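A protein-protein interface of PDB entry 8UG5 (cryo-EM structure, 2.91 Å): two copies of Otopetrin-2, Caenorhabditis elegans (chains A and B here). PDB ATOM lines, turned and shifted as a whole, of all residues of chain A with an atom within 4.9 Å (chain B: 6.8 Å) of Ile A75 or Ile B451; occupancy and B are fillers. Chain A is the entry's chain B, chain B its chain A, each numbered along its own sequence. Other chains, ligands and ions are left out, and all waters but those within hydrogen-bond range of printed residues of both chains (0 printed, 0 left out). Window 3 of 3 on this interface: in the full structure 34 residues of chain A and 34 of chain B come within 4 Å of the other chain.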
ATOM      1  N   LEU A  71      -4.986 -15.299 -32.046  1.00  0.00           N
ATOM      2  CA  LEU A  71      -4.412 -16.168 -31.024  1.00  0.00           C
ATOM      3  C   LEU A  71      -4.632 -17.635 -31.360  1.00  0.00           C
ATOM      4  O   LEU A  71      -3.739 -18.466 -31.163  1.00  0.00           O
ATOM      5  CB  LEU A  71      -5.012 -15.838 -29.658  1.00  0.00           C
ATOM      6  CG  LEU A  71      -4.583 -14.522 -29.011  1.00  0.00           C
ATOM      7  CD1 LEU A  71      -5.117 -14.442 -27.599  1.00  0.00           C
ATOM      8  CD2 LEU A  71      -3.077 -14.394 -29.019  1.00  0.00           C
ATOM      9  N   TYR A  72      -5.823 -17.977 -31.856  1.00  0.00           N
ATOM     10  CA  TYR A  72      -6.082 -19.355 -32.261  1.00  0.00           C
ATOM     11  C   TYR A  72      -5.134 -19.785 -33.371  1.00  0.00           C
ATOM     12  O   TYR A  72      -4.546 -20.873 -33.310  1.00  0.00           O
ATOM     13  CB  TYR A  72      -7.540 -19.494 -32.702  1.00  0.00           C
ATOM     14  CG  TYR A  72      -7.844 -20.726 -33.518  1.00  0.00           C
ATOM     15  CD1 TYR A  72      -7.895 -21.980 -32.927  1.00  0.00           C
ATOM     16  CD2 TYR A  72      -8.095 -20.633 -34.879  1.00  0.00           C
ATOM     17  CE1 TYR A  72      -8.179 -23.104 -33.669  1.00  0.00           C
ATOM     18  CE2 TYR A  72      -8.376 -21.752 -35.627  1.00  0.00           C
ATOM     19  CZ  TYR A  72      -8.419 -22.983 -35.019  1.00  0.00           C
ATOM     20  OH  TYR A  72      -8.702 -24.100 -35.764  1.00  0.00           O
ATOM     21  N   ALA A  73      -4.946 -18.927 -34.374  1.00  0.00           N
ATOM     22  CA  ALA A  73      -4.021 -19.240 -35.457  1.00  0.00           C
ATOM     23  C   ALA A  73      -2.588 -19.343 -34.956  1.00  0.00           C
ATOM     24  O   ALA A  73      -1.837 -20.212 -35.400  1.00  0.00           O
ATOM     25  CB  ALA A  73      -4.118 -18.188 -36.556  1.00  0.00           C
ATOM     26  N   LEU A  74      -2.185 -18.457 -34.042  1.00  0.00           N
ATOM     27  CA  LEU A  74      -0.831 -18.510 -33.499  1.00  0.00           C
ATOM     28  C   LEU A  74      -0.588 -19.810 -32.748  1.00  0.00           C
ATOM     29  O   LEU A  74       0.438 -20.471 -32.952  1.00  0.00           O
ATOM     30  CB  LEU A  74      -0.592 -17.313 -32.583  1.00  0.00           C
ATOM     31  CG  LEU A  74       0.776 -17.193 -31.913  1.00  0.00           C
ATOM     32  CD1 LEU A  74       1.895 -17.307 -32.929  1.00  0.00           C
ATOM     33  CD2 LEU A  74       0.869 -15.885 -31.159  1.00  0.00           C
ATOM     34  N   ILE A  75      -1.530 -20.199 -31.887  1.00  0.00           N
ATOM     35  CA  ILE A  75      -1.395 -21.448 -31.144  1.00  0.00           C
ATOM     36  C   ILE A  75      -1.321 -22.624 -32.103  1.00  0.00           C
ATOM     37  O   ILE A  75      -0.464 -23.503 -31.971  1.00  0.00           O
ATOM     38  CB  ILE A  75      -2.562 -21.623 -30.158  1.00  0.00           C
ATOM     39  CG1 ILE A  75      -2.588 -20.504 -29.125  1.00  0.00           C
ATOM     40  CG2 ILE A  75      -2.480 -22.971 -29.474  1.00  0.00           C
ATOM     41  CD1 ILE A  75      -3.895 -20.441 -28.393  1.00  0.00           C
ATOM     42  N   LEU A  76      -2.226 -22.659 -33.081  1.00  0.00           N
ATOM     43  CA  LEU A  76      -2.311 -23.821 -33.952  1.00  0.00           C
ATOM     44  C   LEU A  76      -1.103 -23.900 -34.876  1.00  0.00           C
ATOM     45  O   LEU A  76      -0.609 -24.993 -35.165  1.00  0.00           O
ATOM     46  CB  LEU A  76      -3.621 -23.778 -34.733  1.00  0.00           C
ATOM     47  CG  LEU A  76      -4.006 -25.003 -35.549  1.00  0.00           C
ATOM     48  CD1 LEU A  76      -4.077 -26.210 -34.647  1.00  0.00           C
ATOM     49  CD2 LEU A  76      -5.357 -24.752 -36.177  1.00  0.00           C
ATOM     50  N   THR A  77      -0.588 -22.751 -35.316  1.00  0.00           N
ATOM     51  CA  THR A  77       0.620 -22.728 -36.132  1.00  0.00           C
ATOM     52  C   THR A  77       1.841 -23.175 -35.336  1.00  0.00           C
ATOM     53  O   THR A  77       2.661 -23.950 -35.841  1.00  0.00           O
ATOM     54  CB  THR A  77       0.836 -21.329 -36.701  1.00  0.00           C
ATOM     55  OG1 THR A  77      -0.327 -20.933 -37.435  1.00  0.00           O
ATOM     56  CG2 THR A  77       2.038 -21.302 -37.619  1.00  0.00           C
ATOM     57  N   ILE A  78       1.978 -22.708 -34.094  1.00  0.00           N
ATOM     58  CA  ILE A  78       3.104 -23.144 -33.272  1.00  0.00           C
ATOM     59  C   ILE A  78       3.014 -24.638 -32.989  1.00  0.00           C
ATOM     60  O   ILE A  78       4.016 -25.358 -33.058  1.00  0.00           O
ATOM     61  CB  ILE A  78       3.166 -22.320 -31.973  1.00  0.00           C
ATOM     62  CG1 ILE A  78       3.616 -20.892 -32.273  1.00  0.00           C
ATOM     63  CG2 ILE A  78       4.088 -22.981 -30.967  1.00  0.00           C
ATOM     64  CD1 ILE A  78       3.626 -19.998 -31.064  1.00  0.00           C
ATOM     65  N   ILE A  79       1.815 -25.128 -32.671  1.00  0.00           N
ATOM     66  CA  ILE A  79       1.626 -26.551 -32.410  1.00  0.00           C
ATOM     67  C   ILE A  79       1.932 -27.365 -33.659  1.00  0.00           C
ATOM     68  O   ILE A  79       2.564 -28.426 -33.585  1.00  0.00           O
ATOM     69  CB  ILE A  79       0.199 -26.808 -31.893  1.00  0.00           C
ATOM     70  CG1 ILE A  79       0.083 -26.387 -30.430  1.00  0.00           C
ATOM     71  CG2 ILE A  79      -0.193 -28.265 -32.063  1.00  0.00           C
ATOM     72  CD1 ILE A  79      -1.323 -26.433 -29.902  1.00  0.00           C
ATOM     73  N   SER A  80       1.493 -26.885 -34.823  1.00  0.00           N
ATOM     74  CA  SER A  80       1.782 -27.567 -36.077  1.00  0.00           C
ATOM     75  C   SER A  80       3.279 -27.622 -36.333  1.00  0.00           C
ATOM     76  O   SER A  80       3.808 -28.659 -36.743  1.00  0.00           O
ATOM     77  CB  SER A  80       1.073 -26.860 -37.226  1.00  0.00           C
ATOM     78  OG  SER A  80      -0.329 -26.870 -37.041  1.00  0.00           O
ATOM     79  N   GLY B 446       6.508 -12.645 -25.759  1.00  0.00           N
ATOM     80  CA  GLY B 446       6.465 -13.474 -24.566  1.00  0.00           C
ATOM     81  C   GLY B 446       5.521 -14.651 -24.712  1.00  0.00           C
ATOM     82  O   GLY B 446       5.833 -15.768 -24.294  1.00  0.00           O
ATOM     83  N   LEU B 447       4.363 -14.422 -25.328  1.00  0.00           N
ATOM     84  CA  LEU B 447       3.377 -15.477 -25.505  1.00  0.00           C
ATOM     85  C   LEU B 447       3.866 -16.540 -26.476  1.00  0.00           C
ATOM     86  O   LEU B 447       3.582 -17.725 -26.291  1.00  0.00           O
ATOM     87  CB  LEU B 447       2.061 -14.877 -25.991  1.00  0.00           C
ATOM     88  CG  LEU B 447       0.943 -15.874 -26.283  1.00  0.00           C
ATOM     89  CD1 LEU B 447       0.607 -16.669 -25.040  1.00  0.00           C
ATOM     90  CD2 LEU B 447      -0.277 -15.158 -26.814  1.00  0.00           C
ATOM     91  N   ILE B 448       4.576 -16.137 -27.529  1.00  0.00           N
ATOM     92  CA  ILE B 448       5.137 -17.108 -28.462  1.00  0.00           C
ATOM     93  C   ILE B 448       6.153 -17.980 -27.749  1.00  0.00           C
ATOM     94  O   ILE B 448       6.160 -19.209 -27.904  1.00  0.00           O
ATOM     95  CB  ILE B 448       5.754 -16.394 -29.677  1.00  0.00           C
ATOM     96  CG1 ILE B 448       4.663 -15.830 -30.582  1.00  0.00           C
ATOM     97  CG2 ILE B 448       6.629 -17.348 -30.465  1.00  0.00           C
ATOM     98  CD1 ILE B 448       5.183 -14.897 -31.640  1.00  0.00           C
ATOM     99  N   GLY B 449       7.021 -17.362 -26.944  1.00  0.00           N
ATOM    100  CA  GLY B 449       7.944 -18.150 -26.143  1.00  0.00           C
ATOM    101  C   GLY B 449       7.227 -19.112 -25.216  1.00  0.00           C
ATOM    102  O   GLY B 449       7.613 -20.278 -25.095  1.00  0.00           O
ATOM    103  N   GLU B 450       6.158 -18.644 -24.568  1.00  0.00           N
ATOM    104  CA  GLU B 450       5.421 -19.487 -23.631  1.00  0.00           C
ATOM    105  C   GLU B 450       4.742 -20.654 -24.336  1.00  0.00           C
ATOM    106  O   GLU B 450       4.788 -21.792 -23.853  1.00  0.00           O
ATOM    107  CB  GLU B 450       4.387 -18.653 -22.880  1.00  0.00           C
ATOM    108  CG  GLU B 450       4.978 -17.672 -21.893  1.00  0.00           C
ATOM    109  CD  GLU B 450       5.063 -18.236 -20.496  1.00  0.00           C
ATOM    110  OE1 GLU B 450       4.722 -19.421 -20.314  1.00  0.00           O
ATOM    111  OE2 GLU B 450       5.473 -17.495 -19.581  1.00  0.00           O
ATOM    112  N   ILE B 451       4.091 -20.388 -25.468  1.00  0.00           N
ATOM    113  CA  ILE B 451       3.397 -21.439 -26.203  1.00  0.00           C
ATOM    114  C   ILE B 451       4.390 -22.459 -26.731  1.00  0.00           C
ATOM    115  O   ILE B 451       4.140 -23.666 -26.683  1.00  0.00           O
ATOM    116  CB  ILE B 451       2.552 -20.835 -27.338  1.00  0.00           C
ATOM    117  CG1 ILE B 451       1.426 -19.977 -26.772  1.00  0.00           C
ATOM    118  CG2 ILE B 451       1.961 -21.929 -28.202  1.00  0.00           C
ATOM    119  CD1 ILE B 451       0.689 -19.193 -27.822  1.00  0.00           C
ATOM    120  N   LEU B 452       5.566 -22.066 -27.197  1.00  0.00           N
ATOM    121  CA  LEU B 452       6.564 -23.064 -27.657  1.00  0.00           C
ATOM    122  C   LEU B 452       7.001 -23.867 -26.464  1.00  0.00           C
ATOM    123  O   LEU B 452       7.039 -25.093 -26.546  1.00  0.00           O
ATOM    124  CB  LEU B 452       7.796 -22.382 -28.256  1.00  0.00           C
ATOM    125  CG  LEU B 452       8.494 -23.105 -29.398  1.00  0.00           C
ATOM    126  CD1 LEU B 452       7.508 -23.926 -30.203  1.00  0.00           C
ATOM    127  CD2 LEU B 452       9.205 -22.108 -30.291  1.00  0.00           C
ATOM    128  N   TYR B 453       7.318 -23.169 -25.400  1.00  0.00           N
ATOM    129  CA  TYR B 453       7.812 -23.925 -24.255  1.00  0.00           C
ATOM    130  C   TYR B 453       6.802 -24.978 -23.816  1.00  0.00           C
ATOM    131  O   TYR B 453       7.158 -26.138 -23.583  1.00  0.00           O
ATOM    132  CB  TYR B 453       8.131 -22.968 -23.106  1.00  0.00           C
ATOM    133  CG  TYR B 453       8.526 -23.653 -21.821  1.00  0.00           C
ATOM    134  CD1 TYR B 453       9.759 -24.272 -21.696  1.00  0.00           C
ATOM    135  CD2 TYR B 453       7.665 -23.686 -20.734  1.00  0.00           C
ATOM    136  CE1 TYR B 453      10.127 -24.901 -20.527  1.00  0.00           C
ATOM    137  CE2 TYR B 453       8.024 -24.316 -19.560  1.00  0.00           C
ATOM    138  CZ  TYR B 453       9.256 -24.920 -19.464  1.00  0.00           C
ATOM    139  OH  TYR B 453       9.622 -25.546 -18.297  1.00  0.00           O
ATOM    140  N   CYS B 454       5.529 -24.593 -23.717  1.00  0.00           N
ATOM    141  CA  CYS B 454       4.501 -25.531 -23.280  1.00  0.00           C
ATOM    142  C   CYS B 454       4.305 -26.657 -24.288  1.00  0.00           C
ATOM    143  O   CYS B 454       4.171 -27.824 -23.904  1.00  0.00           O
ATOM    144  CB  CYS B 454       3.189 -24.789 -23.040  1.00  0.00           C
ATOM    145  SG  CYS B 454       3.227 -23.645 -21.650  1.00  0.00           S
ATOM    146  N   ALA B 455       4.292 -26.328 -25.583  1.00  0.00           N
ATOM    147  CA  ALA B 455       4.126 -27.349 -26.608  1.00  0.00           C
ATOM    148  C   ALA B 455       5.301 -28.317 -26.624  1.00  0.00           C
ATOM    149  O   ALA B 455       5.107 -29.529 -26.754  1.00  0.00           O
ATOM    150  CB  ALA B 455       3.952 -26.692 -27.975  1.00  0.00           C
ATOM    151  N   VAL B 456       6.527 -27.805 -26.490  1.00  0.00           N
ATOM    152  CA  VAL B 456       7.695 -28.680 -26.484  1.00  0.00           C
ATOM    153  C   VAL B 456       7.698 -29.556 -25.238  1.00  0.00           C
ATOM    154  O   VAL B 456       8.068 -30.734 -25.294  1.00  0.00           O
ATOM    155  CB  VAL B 456       8.987 -27.849 -26.606  1.00  0.00           C
ATOM    156  CG1 VAL B 456      10.205 -28.718 -26.371  1.00  0.00           C
ATOM    157  CG2 VAL B 456       9.066 -27.197 -27.978  1.00  0.00           C
ATOM    158  N   GLY B 457       7.276 -29.006 -24.097  1.00  0.00           N
ATOM    159  CA  GLY B 457       7.171 -29.822 -22.898  1.00  0.00           C
ATOM    160  C   GLY B 457       6.151 -30.934 -23.039  1.00  0.00           C
ATOM    161  O   GLY B 457       6.409 -32.081 -22.659  1.00  0.00           O
ATOM    162  N   MET B 484      -0.428 -23.358 -20.741  1.00  0.00           N
ATOM    163  CA  MET B 484      -0.712 -22.809 -22.065  1.00  0.00           C
ATOM    164  C   MET B 484      -2.057 -22.095 -22.084  1.00  0.00           C
ATOM    165  O   MET B 484      -2.176 -20.977 -22.606  1.00  0.00           O
ATOM    166  CB  MET B 484      -0.686 -23.917 -23.118  1.00  0.00           C
ATOM    167  CG  MET B 484      -0.856 -23.402 -24.538  1.00  0.00           C
ATOM    168  SD  MET B 484      -0.820 -24.688 -25.797  1.00  0.00           S
ATOM    169  CE  MET B 484       0.911 -25.131 -25.782  1.00  0.00           C
ATOM    170  N   VAL B 487      -1.706 -18.786 -20.121  1.00  0.00           N
ATOM    171  CA  VAL B 487      -0.962 -17.714 -20.776  1.00  0.00           C
ATOM    172  C   VAL B 487      -1.759 -17.155 -21.946  1.00  0.00           C
ATOM    173  O   VAL B 487      -1.772 -15.942 -22.172  1.00  0.00           O
ATOM    174  CB  VAL B 487       0.446 -18.176 -21.206  1.00  0.00           C
ATOM    175  CG1 VAL B 487       1.258 -18.610 -20.001  1.00  0.00           C
ATOM    176  CG2 VAL B 487       0.392 -19.272 -22.253  1.00  0.00           C
ATOM    177  N   VAL B 488      -2.475 -18.011 -22.680  1.00  0.00           N
ATOM    178  CA  VAL B 488      -3.259 -17.522 -23.811  1.00  0.00           C
ATOM    179  C   VAL B 488      -4.439 -16.680 -23.332  1.00  0.00           C
ATOM    180  O   VAL B 488      -4.698 -15.587 -23.855  1.00  0.00           O
ATOM    181  CB  VAL B 488      -3.715 -18.696 -24.690  1.00  0.00           C
ATOM    182  CG1 VAL B 488      -4.729 -18.230 -25.707  1.00  0.00           C
ATOM    183  CG2 VAL B 488      -2.517 -19.312 -25.368  1.00  0.00           C
ATOM    184  N   LEU B 561       9.922 -16.632 -21.035  1.00  0.00           N
ATOM    185  CA  LEU B 561       8.878 -16.926 -20.056  1.00  0.00           C
ATOM    186  C   LEU B 561       8.818 -15.850 -18.975  1.00  0.00           C
ATOM    187  O   LEU B 561       7.759 -15.258 -18.710  1.00  0.00           O
ATOM    188  CB  LEU B 561       9.148 -18.289 -19.427  1.00  0.00           C
ATOM    189  CG  LEU B 561       9.328 -19.469 -20.383  1.00  0.00           C
ATOM    190  CD1 LEU B 561       9.731 -20.713 -19.618  1.00  0.00           C
ATOM    191  CD2 LEU B 561       8.072 -19.716 -21.186  1.00  0.00           C
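Of chain B, only Ile B451 and Val B488 come within 4 Å of Ile A75.
Printed residues of chain B within 4 Å of Ile A78: Ile B451 and Leu B452.
Ile B451 touches just these residues of chain A: Ile A75 and Ile A78.
Of the printed residues of chain A, Leu B452 touches Ile A78 (3.6 Å).
The nearest printed residue of chain A that does not touch Ile B448 is Ile A78 (4.05 Å).
Among the printed residues, merely in contact across the chains: Ile A75 with Val B488, Ile A78 with Leu B452, Ile A78 with Ile B451, Leu A71 with Leu B447, Ile A75 with Ile B451, Leu A74 with Ile B448 and Leu A71 with Val B488.
No position is printed for both chains.
Of the 16 printed residues of chain B, 5 touch a printed residue of chain A.
Hydrophobic or aromatic side chains of chain B within 4 Å of the printed part of chain A: Leu B447, Ile B448, Ile B451, Leu B452 and Val B488.
Hydrophobic or aromatic side chains of chain A within 4 Å of the printed part of chain B: Leu A71, Leu A74, Ile A75 and Ile A78.
Among the printed residues, no Asp or Glu carboxylate lies within 4 Å of a Lys or Arg side-chain nitrogen of the other chain.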
